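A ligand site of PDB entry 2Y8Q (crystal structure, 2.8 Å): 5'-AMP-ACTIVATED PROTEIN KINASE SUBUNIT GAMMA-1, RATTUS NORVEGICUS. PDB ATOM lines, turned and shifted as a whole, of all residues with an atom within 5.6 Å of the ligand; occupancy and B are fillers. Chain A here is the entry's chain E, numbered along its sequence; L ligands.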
ATOM      1  N   ARG A  69      37.625  -5.875  26.105  1.00  0.00           N
ATOM      2  CA  ARG A  69      36.460  -6.061  26.954  1.00  0.00           C
ATOM      3  C   ARG A  69      35.197  -5.417  26.386  1.00  0.00           C
ATOM      4  O   ARG A  69      34.090  -5.771  26.774  1.00  0.00           O
ATOM      5  CB  ARG A  69      36.734  -5.619  28.400  1.00  0.00           C
ATOM      6  CG  ARG A  69      38.171  -5.904  28.869  1.00  0.00           C
ATOM      7  CD  ARG A  69      38.281  -6.472  30.285  1.00  0.00           C
ATOM      8  NE  ARG A  69      37.954  -5.507  31.345  1.00  0.00           N
ATOM      9  CZ  ARG A  69      37.800  -5.818  32.637  1.00  0.00           C
ATOM     10  NH1 ARG A  69      37.952  -7.076  33.065  1.00  0.00           N
ATOM     11  NH2 ARG A  69      37.501  -4.870  33.523  1.00  0.00           N
ATOM     12  N   ALA A  70      35.342  -4.498  25.439  1.00  0.00           N
ATOM     13  CA  ALA A  70      34.186  -3.798  24.877  1.00  0.00           C
ATOM     14  C   ALA A  70      34.400  -3.460  23.412  1.00  0.00           C
ATOM     15  O   ALA A  70      35.527  -3.274  22.984  1.00  0.00           O
ATOM     16  CB  ALA A  70      33.918  -2.534  25.665  1.00  0.00           C
ATOM     17  N   GLY A  83      25.635   1.903  19.471  1.00  0.00           N
ATOM     18  CA  GLY A  83      25.724   1.307  20.807  1.00  0.00           C
ATOM     19  C   GLY A  83      27.057   0.666  21.148  1.00  0.00           C
ATOM     20  O   GLY A  83      28.076   0.994  20.537  1.00  0.00           O
ATOM     21  N   MET A  84      27.040  -0.228  22.138  1.00  0.00           N
ATOM     22  CA  MET A  84      28.237  -0.910  22.647  1.00  0.00           C
ATOM     23  C   MET A  84      27.891  -2.352  23.013  1.00  0.00           C
ATOM     24  O   MET A  84      26.791  -2.629  23.501  1.00  0.00           O
ATOM     25  CB  MET A  84      28.780  -0.204  23.908  1.00  0.00           C
ATOM     26  CG  MET A  84      29.589   1.055  23.652  1.00  0.00           C
ATOM     27  SD  MET A  84      31.352   0.740  23.454  1.00  0.00           S
ATOM     28  CE  MET A  84      31.815   2.139  22.449  1.00  0.00           C
ATOM     29  N   LEU A  85      28.846  -3.257  22.787  1.00  0.00           N
ATOM     30  CA  LEU A  85      28.670  -4.657  23.164  1.00  0.00           C
ATOM     31  C   LEU A  85      29.707  -5.050  24.203  1.00  0.00           C
ATOM     32  O   LEU A  85      30.889  -5.160  23.900  1.00  0.00           O
ATOM     33  CB  LEU A  85      28.820  -5.554  21.940  1.00  0.00           C
ATOM     34  CG  LEU A  85      28.321  -6.988  22.087  1.00  0.00           C
ATOM     35  CD1 LEU A  85      26.849  -7.040  21.812  1.00  0.00           C
ATOM     36  CD2 LEU A  85      29.074  -7.908  21.145  1.00  0.00           C
ATOM     37  N   THR A  86      29.265  -5.230  25.439  1.00  0.00           N
ATOM     38  CA  THR A  86      30.177  -5.502  26.540  1.00  0.00           C
ATOM     39  C   THR A  86      29.949  -6.891  27.110  1.00  0.00           C
ATOM     40  O   THR A  86      29.122  -7.647  26.613  1.00  0.00           O
ATOM     41  CB  THR A  86      30.046  -4.451  27.641  1.00  0.00           C
ATOM     42  OG1 THR A  86      28.820  -4.623  28.339  1.00  0.00           O
ATOM     43  CG2 THR A  86      30.091  -3.053  27.044  1.00  0.00           C
ATOM     44  N   ILE A  87      30.723  -7.221  28.142  1.00  0.00           N
ATOM     45  CA  ILE A  87      30.657  -8.508  28.845  1.00  0.00           C
ATOM     46  C   ILE A  87      29.300  -8.690  29.534  1.00  0.00           C
ATOM     47  O   ILE A  87      28.799  -9.806  29.657  1.00  0.00           O
ATOM     48  CB  ILE A  87      31.789  -8.635  29.926  1.00  0.00           C
ATOM     49  CG1 ILE A  87      33.122  -8.052  29.422  1.00  0.00           C
ATOM     50  CG2 ILE A  87      31.926 -10.079  30.447  1.00  0.00           C
ATOM     51  CD1 ILE A  87      33.818  -8.849  28.316  1.00  0.00           C
ATOM     52  N   THR A  88      28.747  -7.579  30.012  1.00  0.00           N
ATOM     53  CA  THR A  88      27.427  -7.558  30.648  1.00  0.00           C
ATOM     54  C   THR A  88      26.351  -8.021  29.671  1.00  0.00           C
ATOM     55  O   THR A  88      25.419  -8.744  30.042  1.00  0.00           O
ATOM     56  CB  THR A  88      27.134  -6.158  31.233  1.00  0.00           C
ATOM     57  OG1 THR A  88      27.865  -6.016  32.461  1.00  0.00           O
ATOM     58  CG2 THR A  88      25.679  -5.940  31.523  1.00  0.00           C
ATOM     59  N   ASP A  89      26.496  -7.636  28.412  1.00  0.00           N
ATOM     60  CA  ASP A  89      25.626  -8.108  27.358  1.00  0.00           C
ATOM     61  C   ASP A  89      25.818  -9.603  27.149  1.00  0.00           C
ATOM     62  O   ASP A  89      24.843 -10.355  27.125  1.00  0.00           O
ATOM     63  CB  ASP A  89      25.913  -7.346  26.058  1.00  0.00           C
ATOM     64  CG  ASP A  89      25.728  -5.857  26.226  1.00  0.00           C
ATOM     65  OD1 ASP A  89      24.603  -5.434  26.587  1.00  0.00           O
ATOM     66  OD2 ASP A  89      26.703  -5.094  26.017  1.00  0.00           O
ATOM     67  N   ASN A  92      23.902 -11.202  29.907  1.00  0.00           N
ATOM     68  CA  ASN A  92      22.472 -11.183  29.682  1.00  0.00           C
ATOM     69  C   ASN A  92      22.034 -12.229  28.649  1.00  0.00           C
ATOM     70  O   ASN A  92      21.036 -12.944  28.833  1.00  0.00           O
ATOM     71  CB  ASN A  92      22.016  -9.782  29.259  1.00  0.00           C
ATOM     72  CG  ASN A  92      21.973  -8.803  30.421  1.00  0.00           C
ATOM     73  OD1 ASN A  92      21.588  -9.156  31.530  1.00  0.00           O
ATOM     74  ND2 ASN A  92      22.360  -7.556  30.160  1.00  0.00           N
ATOM     75  N   LYS A 126      18.185   3.197  24.887  1.00  0.00           N
ATOM     76  CA  LYS A 126      19.596   3.277  25.306  1.00  0.00           C
ATOM     77  C   LYS A 126      20.498   3.849  24.202  1.00  0.00           C
ATOM     78  O   LYS A 126      21.262   3.104  23.581  1.00  0.00           O
ATOM     79  CB  LYS A 126      20.134   1.913  25.769  1.00  0.00           C
ATOM     80  CG  LYS A 126      19.584   1.403  27.098  1.00  0.00           C
ATOM     81  CD  LYS A 126      19.863   2.362  28.257  1.00  0.00           C
ATOM     82  CE  LYS A 126      18.948   2.045  29.437  1.00  0.00           C
ATOM     83  NZ  LYS A 126      18.839   3.202  30.362  1.00  0.00           N
ATOM     84  N   PRO A 127      20.412   5.163  23.938  1.00  0.00           N
ATOM     85  CA  PRO A 127      21.309   5.743  22.948  1.00  0.00           C
ATOM     86  C   PRO A 127      22.771   5.611  23.374  1.00  0.00           C
ATOM     87  O   PRO A 127      23.076   5.684  24.567  1.00  0.00           O
ATOM     88  CB  PRO A 127      20.901   7.218  22.909  1.00  0.00           C
ATOM     89  CG  PRO A 127      20.250   7.476  24.212  1.00  0.00           C
ATOM     90  CD  PRO A 127      19.560   6.199  24.573  1.00  0.00           C
ATOM     91  N   LEU A 128      23.663   5.379  22.410  1.00  0.00           N
ATOM     92  CA  LEU A 128      25.088   5.377  22.683  1.00  0.00           C
ATOM     93  C   LEU A 128      25.488   6.698  23.320  1.00  0.00           C
ATOM     94  O   LEU A 128      25.099   7.760  22.828  1.00  0.00           O
ATOM     95  CB  LEU A 128      25.899   5.138  21.407  1.00  0.00           C
ATOM     96  CG  LEU A 128      27.419   5.348  21.491  1.00  0.00           C
ATOM     97  CD1 LEU A 128      28.109   4.225  22.264  1.00  0.00           C
ATOM     98  CD2 LEU A 128      28.013   5.463  20.117  1.00  0.00           C
ATOM     99  N   VAL A 129      26.229   6.631  24.416  1.00  0.00           N
ATOM    100  CA  VAL A 129      26.842   7.832  24.984  1.00  0.00           C
ATOM    101  C   VAL A 129      28.330   7.837  24.653  1.00  0.00           C
ATOM    102  O   VAL A 129      29.013   6.828  24.809  1.00  0.00           O
ATOM    103  CB  VAL A 129      26.537   8.061  26.522  1.00  0.00           C
ATOM    104  CG1 VAL A 129      25.299   7.314  26.963  1.00  0.00           C
ATOM    105  CG2 VAL A 129      27.700   7.673  27.388  1.00  0.00           C
ATOM    106  N   CYS A 130      28.803   8.969  24.153  1.00  0.00           N
ATOM    107  CA  CYS A 130      30.191   9.126  23.763  1.00  0.00           C
ATOM    108  C   CYS A 130      30.670  10.499  24.198  1.00  0.00           C
ATOM    109  O   CYS A 130      29.881  11.308  24.684  1.00  0.00           O
ATOM    110  CB  CYS A 130      30.319   9.024  22.249  1.00  0.00           C
ATOM    111  SG  CYS A 130      29.541  10.415  21.405  1.00  0.00           S
ATOM    112  N   LYS A 148      25.626   5.295  34.493  1.00  0.00           N
ATOM    113  CA  LYS A 148      25.852   4.014  35.170  1.00  0.00           C
ATOM    114  C   LYS A 148      26.567   3.005  34.275  1.00  0.00           C
ATOM    115  O   LYS A 148      26.099   1.887  34.049  1.00  0.00           O
ATOM    116  CB  LYS A 148      24.549   3.447  35.757  1.00  0.00           C
ATOM    117  CG  LYS A 148      24.057   4.232  36.953  1.00  0.00           C
ATOM    118  CD  LYS A 148      22.835   3.594  37.557  1.00  0.00           C
ATOM    119  CE  LYS A 148      22.261   4.480  38.646  1.00  0.00           C
ATOM    120  NZ  LYS A 148      21.274   3.739  39.494  1.00  0.00           N
ATOM    121  N   ILE A 149      27.727   3.414  33.804  1.00  0.00           N
ATOM    122  CA  ILE A 149      28.421   2.731  32.727  1.00  0.00           C
ATOM    123  C   ILE A 149      29.939   2.563  32.994  1.00  0.00           C
ATOM    124  O   ILE A 149      30.522   3.284  33.819  1.00  0.00           O
ATOM    125  CB  ILE A 149      28.093   3.472  31.387  1.00  0.00           C
ATOM    126  CG1 ILE A 149      27.742   2.485  30.297  1.00  0.00           C
ATOM    127  CG2 ILE A 149      29.098   4.589  31.032  1.00  0.00           C
ATOM    128  CD1 ILE A 149      26.354   1.945  30.474  1.00  0.00           C
ATOM    129  N   HIS A 150      30.551   1.596  32.313  1.00  0.00           N
ATOM    130  CA  HIS A 150      31.978   1.293  32.501  1.00  0.00           C
ATOM    131  C   HIS A 150      32.841   1.616  31.282  1.00  0.00           C
ATOM    132  O   HIS A 150      34.063   1.555  31.365  1.00  0.00           O
ATOM    133  CB  HIS A 150      32.154  -0.171  32.901  1.00  0.00           C
ATOM    134  CG  HIS A 150      31.653  -0.487  34.273  1.00  0.00           C
ATOM    135  ND1 HIS A 150      30.361  -0.881  34.522  1.00  0.00           N
ATOM    136  CD2 HIS A 150      32.269  -0.457  35.478  1.00  0.00           C
ATOM    137  CE1 HIS A 150      30.196  -1.082  35.820  1.00  0.00           C
ATOM    138  NE2 HIS A 150      31.342  -0.829  36.416  1.00  0.00           N
ATOM    139  N   ARG A 151      32.233   1.926  30.145  1.00  0.00           N
ATOM    140  CA  ARG A 151      32.966   2.238  28.918  1.00  0.00           C
ATOM    141  C   ARG A 151      32.471   3.560  28.345  1.00  0.00           C
ATOM    142  O   ARG A 151      31.252   3.810  28.283  1.00  0.00           O
ATOM    143  CB  ARG A 151      32.770   1.127  27.873  1.00  0.00           C
ATOM    144  CG  ARG A 151      32.749  -0.281  28.432  1.00  0.00           C
ATOM    145  CD  ARG A 151      34.147  -0.757  28.736  1.00  0.00           C
ATOM    146  NE  ARG A 151      34.151  -1.827  29.752  1.00  0.00           N
ATOM    147  CZ  ARG A 151      35.250  -2.468  30.151  1.00  0.00           C
ATOM    148  NH1 ARG A 151      36.439  -2.171  29.619  1.00  0.00           N
ATOM    149  NH2 ARG A 151      35.167  -3.417  31.084  1.00  0.00           N
ATOM    150  N   LEU A 152      33.401   4.405  27.923  1.00  0.00           N
ATOM    151  CA  LEU A 152      33.046   5.696  27.344  1.00  0.00           C
ATOM    152  C   LEU A 152      33.863   5.936  26.083  1.00  0.00           C
ATOM    153  O   LEU A 152      35.045   6.270  26.161  1.00  0.00           O
ATOM    154  CB  LEU A 152      33.267   6.827  28.355  1.00  0.00           C
ATOM    155  CG  LEU A 152      32.772   8.222  27.991  1.00  0.00           C
ATOM    156  CD1 LEU A 152      31.277   8.232  27.711  1.00  0.00           C
ATOM    157  CD2 LEU A 152      33.089   9.203  29.089  1.00  0.00           C
ATOM    158  N   PRO A 153      33.249   5.718  24.916  1.00  0.00           N
ATOM    159  CA  PRO A 153      33.963   5.945  23.659  1.00  0.00           C
ATOM    160  C   PRO A 153      34.305   7.406  23.450  1.00  0.00           C
ATOM    161  O   PRO A 153      33.465   8.281  23.643  1.00  0.00           O
ATOM    162  CB  PRO A 153      32.952   5.507  22.590  1.00  0.00           C
ATOM    163  CG  PRO A 153      31.627   5.465  23.275  1.00  0.00           C
ATOM    164  CD  PRO A 153      31.926   5.125  24.705  1.00  0.00           C
ATOM    165  N   SER A 225      29.637  -6.198  39.109  1.00  0.00           N
ATOM    166  CA  SER A 225      30.618  -6.743  38.177  1.00  0.00           C
ATOM    167  C   SER A 225      31.475  -7.905  38.704  1.00  0.00           C
ATOM    168  O   SER A 225      32.084  -8.628  37.920  1.00  0.00           O
ATOM    169  CB  SER A 225      31.440  -5.631  37.499  1.00  0.00           C
ATOM    170  OG  SER A 225      32.615  -5.393  38.196  1.00  0.00           O
ATOM    171  N   LYS A 242      32.563 -11.193  36.331  1.00  0.00           N
ATOM    172  CA  LYS A 242      31.918 -11.191  35.022  1.00  0.00           C
ATOM    173  C   LYS A 242      32.905 -11.541  33.887  1.00  0.00           C
ATOM    174  O   LYS A 242      32.568 -12.310  32.998  1.00  0.00           O
ATOM    175  CB  LYS A 242      31.281  -9.821  34.765  1.00  0.00           C
ATOM    176  CG  LYS A 242      29.897  -9.632  35.361  1.00  0.00           C
ATOM    177  CD  LYS A 242      29.365  -8.243  35.041  1.00  0.00           C
ATOM    178  CE  LYS A 242      27.851  -8.186  35.129  1.00  0.00           C
ATOM    179  NZ  LYS A 242      27.358  -6.780  35.213  1.00  0.00           N
HETATM  180  P1  LIG L   1      30.752  -3.886  31.376  1.00  0.00           P
HETATM  181  O1  LIG L   1      31.932  -4.286  30.493  1.00  0.00           O
HETATM  182  O2  LIG L   1      29.500  -4.683  31.146  1.00  0.00           O
HETATM  183  O3  LIG L   1      31.144  -3.661  32.827  1.00  0.00           O
HETATM  184  P2  LIG L   1      28.953  -1.687  31.338  1.00  0.00           P
HETATM  185  O4  LIG L   1      29.149  -0.254  30.887  1.00  0.00           O
HETATM  186  O5  LIG L   1      28.663  -1.989  32.777  1.00  0.00           O
HETATM  187  O6  LIG L   1      30.262  -2.457  30.813  1.00  0.00           O
HETATM  188  O7  LIG L   1      27.722  -2.293  30.501  1.00  0.00           O
HETATM  189  C1  LIG L   1      26.414  -1.904  30.920  1.00  0.00           C
HETATM  190  C2  LIG L   1      25.422  -1.928  29.752  1.00  0.00           C
HETATM  191  O8  LIG L   1      25.333  -0.648  29.123  1.00  0.00           O
HETATM  192  C3  LIG L   1      25.810  -2.919  28.656  1.00  0.00           C
HETATM  193  O9  LIG L   1      24.603  -3.534  28.202  1.00  0.00           O
HETATM  194  C4  LIG L   1      26.445  -2.073  27.570  1.00  0.00           C
HETATM  195  O10 LIG L   1      26.247  -2.595  26.257  1.00  0.00           O
HETATM  196  C5  LIG L   1      25.783  -0.706  27.751  1.00  0.00           C
HETATM  197  N1  LIG L   1      26.759   0.374  27.467  1.00  0.00           N
HETATM  198  C6  LIG L   1      28.060   0.375  27.833  1.00  0.00           C
HETATM  199  N2  LIG L   1      28.673   1.514  27.409  1.00  0.00           N
HETATM  200  C7  LIG L   1      27.756   2.275  26.776  1.00  0.00           C
HETATM  201  C8  LIG L   1      27.743   3.593  26.105  1.00  0.00           C
HETATM  202  N3  LIG L   1      28.875   4.335  26.023  1.00  0.00           N
HETATM  203  N4  LIG L   1      26.571   4.017  25.574  1.00  0.00           N
HETATM  204  C9  LIG L   1      25.458   3.267  25.647  1.00  0.00           C
HETATM  205  N5  LIG L   1      25.395   2.055  26.247  1.00  0.00           N
HETATM  206  C10 LIG L   1      26.490   1.512  26.822  1.00  0.00           C
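Residues that only touch the ligand: Ile 149, Pro 153, Leu 128, Pro 127 and Ile 87. 12 residues have an atom within 4 Å of the ligand: Met 84, Thr 86, Ile 87, Thr 88, Asp 89, Pro 127, Leu 128, Val 129, Ile 149, His 150, Arg 151 and Pro 153. The nearest printed residue that does not touch the ligand is Leu 85 (4.4 Å).
An oxygen (O2) of the ligand lies close to the backbone NH (N) of Thr 88 (3.2 Å). An oxygen (O2) of the ligand sits at hydrogen-bond distance from the side-chain hydroxyl (OG1) of Thr 88, 2.5 Å away. OD1 of Asp 89 sits at hydrogen-bond distance from O9 of the ligand (2.5 Å). An oxygen (O4) of the ligand sits at hydrogen-bond distance from the backbone NH of His 150 (2.7 Å). An oxygen (O5) of the ligand sits at hydrogen-bond distance from a ring nitrogen (ND1) of His 150 (2.7 Å). N4 of the ligand lies within hydrogen-bond range of N of Val 129 (2.9 Å). The backbone carbonyl oxygen (O) of Val 129 lies within hydrogen-bond range of a nitrogen (N3) of the ligand (2.8 Å). O of Met 84 is in hydrogen-bond range of O10 of the ligand. The side-chain hydroxyl of Thr 86 is in hydrogen-bond range of an oxygen (O2) of the ligand (2.9 Å). N3 of the ligand is in hydrogen-bond range of O of Arg 151. NE of Arg 151 lies within salt-bridge range of O1 of the ligand (3.4 Å).
OG1 of Thr 86 sits close to N of Thr 88, at 3.4 Å. O of Thr 88 lies within hydrogen-bond range of ND2 of Asn 92. OG1 of Thr 88 is in hydrogen-bond range of NZ of Lys 242, at 2.9 Å. The side-chain carboxylate (OD2) of Asp 89 lies within hydrogen-bond range of the backbone NH (N) of Thr 86 (2.6 Å).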
